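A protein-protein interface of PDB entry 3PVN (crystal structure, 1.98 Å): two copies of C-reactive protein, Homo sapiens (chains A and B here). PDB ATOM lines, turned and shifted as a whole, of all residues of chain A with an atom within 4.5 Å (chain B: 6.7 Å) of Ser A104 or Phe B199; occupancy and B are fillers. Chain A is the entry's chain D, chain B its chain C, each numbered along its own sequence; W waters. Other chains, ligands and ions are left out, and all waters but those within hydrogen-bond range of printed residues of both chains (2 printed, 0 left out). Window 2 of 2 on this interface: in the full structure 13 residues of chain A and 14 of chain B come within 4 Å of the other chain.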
ATOM      1  N   GLU A 101      13.108  18.437  23.330  1.00  0.00           N
ATOM      2  CA  GLU A 101      12.231  19.195  24.235  1.00  0.00           C
ATOM      3  C   GLU A 101      12.936  19.363  25.581  1.00  0.00           C
ATOM      4  O   GLU A 101      13.219  18.375  26.274  1.00  0.00           O
ATOM      5  CB  GLU A 101      10.980  18.358  24.515  1.00  0.00           C
ATOM      6  CG  GLU A 101       9.918  19.161  25.301  1.00  0.00           C
ATOM      7  CD  GLU A 101       8.703  18.294  25.712  1.00  0.00           C
ATOM      8  OE1 GLU A 101       8.854  17.049  25.887  1.00  0.00           O
ATOM      9  OE2 GLU A 101       7.619  18.888  25.868  1.00  0.00           O
ATOM     10  N   SER A 102      13.119  20.595  26.005  1.00  0.00           N
ATOM     11  CA  SER A 102      13.712  20.863  27.300  1.00  0.00           C
ATOM     12  C   SER A 102      12.977  20.246  28.485  1.00  0.00           C
ATOM     13  O   SER A 102      13.605  19.725  29.422  1.00  0.00           O
ATOM     14  CB  SER A 102      13.721  22.400  27.556  1.00  0.00           C
ATOM     15  OG  SER A 102      14.488  22.607  28.730  1.00  0.00           O
ATOM     16  N   ALA A 103      11.642  20.313  28.429  1.00  0.00           N
ATOM     17  CA  ALA A 103      10.777  19.899  29.557  1.00  0.00           C
ATOM     18  C   ALA A 103      10.989  18.478  29.945  1.00  0.00           C
ATOM     19  O   ALA A 103      11.098  18.226  31.135  1.00  0.00           O
ATOM     20  CB  ALA A 103       9.208  20.174  29.281  1.00  0.00           C
ATOM     21  N   SER A 104      11.024  17.546  28.960  1.00  0.00           N
ATOM     22  CA  SER A 104      11.282  16.124  29.255  1.00  0.00           C
ATOM     23  C   SER A 104      12.730  15.684  28.985  1.00  0.00           C
ATOM     24  O   SER A 104      13.103  14.585  29.380  1.00  0.00           O
ATOM     25  CB  SER A 104      10.406  15.235  28.370  1.00  0.00           C
ATOM     26  OG  SER A 104      10.650  15.571  26.970  1.00  0.00           O
ATOM     27  N   GLY A 105      13.469  16.467  28.209  1.00  0.00           N
ATOM     28  CA  GLY A 105      14.808  16.038  27.687  1.00  0.00           C
ATOM     29  C   GLY A 105      14.672  15.077  26.526  1.00  0.00           C
ATOM     30  O   GLY A 105      15.695  14.547  26.063  1.00  0.00           O
ATOM     31  N   ILE A 106      13.427  14.848  26.029  1.00  0.00           N
ATOM     32  CA  ILE A 106      13.234  13.807  24.994  1.00  0.00           C
ATOM     33  C   ILE A 106      13.804  14.243  23.645  1.00  0.00           C
ATOM     34  O   ILE A 106      13.493  15.337  23.150  1.00  0.00           O
ATOM     35  CB  ILE A 106      11.746  13.275  24.886  1.00  0.00           C
ATOM     36  CG1 ILE A 106      11.375  12.466  26.126  1.00  0.00           C
ATOM     37  CG2 ILE A 106      11.532  12.467  23.605  1.00  0.00           C
ATOM     38  CD1 ILE A 106       9.819  12.124  26.240  1.00  0.00           C
ATOM     39  N   LYS A 123      17.848  17.664  29.661  1.00  0.00           N
ATOM     40  CA  LYS A 123      16.588  18.077  30.258  1.00  0.00           C
ATOM     41  C   LYS A 123      16.785  19.373  31.082  1.00  0.00           C
ATOM     42  O   LYS A 123      17.741  19.469  31.862  1.00  0.00           O
ATOM     43  CB  LYS A 123      16.092  16.944  31.143  1.00  0.00           C
ATOM     44  CG  LYS A 123      14.703  17.117  31.720  1.00  0.00           C
ATOM     45  CD  LYS A 123      14.424  15.933  32.656  1.00  0.00           C
ATOM     46  CE  LYS A 123      13.023  16.003  33.186  1.00  0.00           C
ATOM     47  NZ  LYS A 123      12.867  14.911  34.197  1.00  0.00           N
ATOM     48  N   ALA B   8       1.657   6.601  24.064  1.00  0.00           N
ATOM     49  CA  ALA B   8       2.523   5.534  24.607  1.00  0.00           C
ATOM     50  C   ALA B   8       3.308   6.115  25.785  1.00  0.00           C
ATOM     51  O   ALA B   8       3.486   7.333  25.877  1.00  0.00           O
ATOM     52  CB  ALA B   8       3.506   5.061  23.493  1.00  0.00           C
ATOM     53  N   PHE B   9       3.733   5.271  26.703  1.00  0.00           N
ATOM     54  CA  PHE B   9       4.560   5.683  27.772  1.00  0.00           C
ATOM     55  C   PHE B   9       6.028   5.609  27.302  1.00  0.00           C
ATOM     56  O   PHE B   9       6.411   4.614  26.615  1.00  0.00           O
ATOM     57  CB  PHE B   9       4.425   4.762  28.985  1.00  0.00           C
ATOM     58  CG  PHE B   9       3.125   4.907  29.702  1.00  0.00           C
ATOM     59  CD1 PHE B   9       2.780   6.107  30.287  1.00  0.00           C
ATOM     60  CD2 PHE B   9       2.207   3.809  29.755  1.00  0.00           C
ATOM     61  CE1 PHE B   9       1.563   6.199  30.982  1.00  0.00           C
ATOM     62  CE2 PHE B   9       1.009   3.923  30.404  1.00  0.00           C
ATOM     63  CZ  PHE B   9       0.692   5.083  31.020  1.00  0.00           C
ATOM     64  N   VAL B  10       6.810   6.616  27.699  1.00  0.00           N
ATOM     65  CA  VAL B  10       8.222   6.761  27.252  1.00  0.00           C
ATOM     66  C   VAL B  10       9.119   6.718  28.486  1.00  0.00           C
ATOM     67  O   VAL B  10       8.923   7.514  29.448  1.00  0.00           O
ATOM     68  CB  VAL B  10       8.487   8.074  26.522  1.00  0.00           C
ATOM     69  CG1 VAL B  10       9.992   8.106  25.908  1.00  0.00           C
ATOM     70  CG2 VAL B  10       7.524   8.247  25.351  1.00  0.00           C
ATOM     71  N   PHE B  11      10.068   5.780  28.486  1.00  0.00           N
ATOM     72  CA  PHE B  11      11.102   5.655  29.528  1.00  0.00           C
ATOM     73  C   PHE B  11      12.452   5.928  28.835  1.00  0.00           C
ATOM     74  O   PHE B  11      13.061   5.015  28.267  1.00  0.00           O
ATOM     75  CB  PHE B  11      11.136   4.288  30.111  1.00  0.00           C
ATOM     76  CG  PHE B  11       9.804   3.775  30.631  1.00  0.00           C
ATOM     77  CD1 PHE B  11       8.876   3.231  29.767  1.00  0.00           C
ATOM     78  CD2 PHE B  11       9.543   3.771  32.010  1.00  0.00           C
ATOM     79  CE1 PHE B  11       7.646   2.719  30.220  1.00  0.00           C
ATOM     80  CE2 PHE B  11       8.319   3.263  32.518  1.00  0.00           C
ATOM     81  CZ  PHE B  11       7.344   2.724  31.603  1.00  0.00           C
ATOM     82  N   PRO B  12      12.883   7.169  28.845  1.00  0.00           N
ATOM     83  CA  PRO B  12      14.012   7.673  28.012  1.00  0.00           C
ATOM     84  C   PRO B  12      15.407   7.304  28.495  1.00  0.00           C
ATOM     85  O   PRO B  12      16.344   7.552  27.773  1.00  0.00           O
ATOM     86  CB  PRO B  12      13.895   9.183  28.103  1.00  0.00           C
ATOM     87  CG  PRO B  12      12.725   9.491  28.993  1.00  0.00           C
ATOM     88  CD  PRO B  12      12.161   8.260  29.536  1.00  0.00           C
ATOM     89  N   GLY B 196       8.488   8.201  38.943  1.00  0.00           N
ATOM     90  CA  GLY B 196       9.754   8.506  38.320  1.00  0.00           C
ATOM     91  C   GLY B 196       9.635   9.132  36.963  1.00  0.00           C
ATOM     92  O   GLY B 196       8.633   9.839  36.628  1.00  0.00           O
ATOM     93  N   GLU B 197      10.669   8.940  36.164  1.00  0.00           N
ATOM     94  CA  GLU B 197      10.761   9.661  34.920  1.00  0.00           C
ATOM     95  C   GLU B 197      10.086   8.904  33.764  1.00  0.00           C
ATOM     96  O   GLU B 197      10.707   8.162  33.010  1.00  0.00           O
ATOM     97  CB  GLU B 197      12.212  10.078  34.643  1.00  0.00           C
ATOM     98  CG  GLU B 197      12.538  11.611  35.058  1.00  0.00           C
ATOM     99  CD  GLU B 197      11.814  12.246  36.332  1.00  0.00           C
ATOM    100  OE1 GLU B 197      11.550  11.616  37.415  1.00  0.00           O
ATOM    101  OE2 GLU B 197      11.546  13.465  36.247  1.00  0.00           O
ATOM    102  N   VAL B 198       8.790   9.072  33.668  1.00  0.00           N
ATOM    103  CA  VAL B 198       8.025   8.445  32.570  1.00  0.00           C
ATOM    104  C   VAL B 198       7.149   9.507  31.926  1.00  0.00           C
ATOM    105  O   VAL B 198       6.518  10.307  32.612  1.00  0.00           O
ATOM    106  CB  VAL B 198       7.153   7.282  33.085  1.00  0.00           C
ATOM    107  CG1 VAL B 198       6.149   7.856  33.950  1.00  0.00           C
ATOM    108  CG2 VAL B 198       6.414   6.552  31.929  1.00  0.00           C
ATOM    109  N   PHE B 199       7.093   9.523  30.603  1.00  0.00           N
ATOM    110  CA  PHE B 199       6.344  10.553  29.908  1.00  0.00           C
ATOM    111  C   PHE B 199       5.249   9.928  29.063  1.00  0.00           C
ATOM    112  O   PHE B 199       5.392   8.781  28.673  1.00  0.00           O
ATOM    113  CB  PHE B 199       7.299  11.355  29.014  1.00  0.00           C
ATOM    114  CG  PHE B 199       8.421  11.990  29.789  1.00  0.00           C
ATOM    115  CD1 PHE B 199       9.625  11.332  29.919  1.00  0.00           C
ATOM    116  CD2 PHE B 199       8.184  13.141  30.587  1.00  0.00           C
ATOM    117  CE1 PHE B 199      10.644  11.850  30.716  1.00  0.00           C
ATOM    118  CE2 PHE B 199       9.225  13.691  31.362  1.00  0.00           C
ATOM    119  CZ  PHE B 199      10.419  13.036  31.448  1.00  0.00           C
ATOM    120  N   THR B 200       4.196  10.677  28.774  1.00  0.00           N
ATOM    121  CA  THR B 200       3.158  10.203  27.824  1.00  0.00           C
ATOM    122  C   THR B 200       3.316  10.993  26.584  1.00  0.00           C
ATOM    123  O   THR B 200       3.349  12.204  26.644  1.00  0.00           O
ATOM    124  CB  THR B 200       1.731  10.429  28.431  1.00  0.00           C
ATOM    125  OG1 THR B 200       1.733   9.753  29.706  1.00  0.00           O
ATOM    126  CG2 THR B 200       0.668   9.767  27.536  1.00  0.00           C
ATOM    127  N   LYS B 201       3.439  10.342  25.440  1.00  0.00           N
ATOM    128  CA  LYS B 201       3.687  11.022  24.181  1.00  0.00           C
ATOM    129  C   LYS B 201       2.913  10.321  23.070  1.00  0.00           C
ATOM    130  O   LYS B 201       2.580   9.201  23.190  1.00  0.00           O
ATOM    131  CB  LYS B 201       5.223  10.907  23.843  1.00  0.00           C
ATOM    132  CG  LYS B 201       6.179  11.800  24.792  1.00  0.00           C
ATOM    133  CD  LYS B 201       5.869  13.269  24.590  1.00  0.00           C
ATOM    134  CE  LYS B 201       6.590  14.205  25.560  1.00  0.00           C
ATOM    135  NZ  LYS B 201       6.226  15.644  25.273  1.00  0.00           N
HETATM  136  O   HOH W   1       5.990  17.970  27.596  1.00  0.00           O
HETATM  137  O   HOH W   2      10.190  15.187  34.527  1.00  0.00           O
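No position is printed for both chains. Of the 5 pairs that touch across the chains among the printed residues, none has its exchanged pair printed and touching as well.
Water W1 bridges the side-chain carboxylate of Glu A101 (2.5 Å) and the side-chain amino group of Lys B201 (3.3 Å). Water W2 bridges NZ of Lys A123 (2.7 Å) and OE2 of Glu B197 (2.8 Å).
Among the printed residues, merely in contact across the chains: Ser A104 with Phe B199 (3.6 Å), Ile A106 with Phe B199 (3.8 Å) and Ile A106 with Lys B201 (3.9 Å).
Hydrophobic or aromatic side chains of chain B that line the printed part of chain A: Phe B199. Along chain B the printed residues that touch a printed residue of chain A span positions 197 to 201. Printed residues of chain A that touch a printed residue of chain B: Glu A101, Ser A104, Ile A106 and Lys A123. Hydrophobic or aromatic side chains of chain A that line the printed part of chain B: Ile A106.
OE2 of Glu B197 is in salt-bridge range of NZ of Lys A123, at 2.8 Å. OE1 of Glu A101 is in salt-bridge range of NZ of Lys B201, at 3.0 Å.
The backbone NH of Ala B8 sits at hydrogen-bond distance from the backbone carbonyl oxygen of Lys B201. The backbone carbonyl oxygen of Phe B199 is in hydrogen-bond range of the backbone NH of Val B10 (2.8 Å). OE1 of Glu A101 is in hydrogen-bond range of OG of Ser A104, at 2.6 Å. The backbone carbonyl oxygen of Ile A106 sits at hydrogen-bond distance from the backbone NH of Glu A101 (3.1 Å). The backbone NH of Ile A106 is in hydrogen-bond range of the side-chain hydroxyl of Ser A104 (3.0 Å).
Printed residues of chain B within 4 Å of Ser A104: Phe B199. Phe B199 touches just these residues of chain A: Ser A104 and Ile A106. Printed residues of chain A within 4 Å of Glu B197: Lys A123. Printed residues of chain B within 4 Å of Glu A101: Lys B201. Printed residues of chain B within 4 Å of Lys A123: Glu B197. Thr B200 touches none of the printed residues of chain A. The nearest residue of chain B that does not touch Ser A104 is Lys B201 (4.5 Å). The nearest printed residue of chain B that does not touch Ile A106 is Val B10 (4.04 Å).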
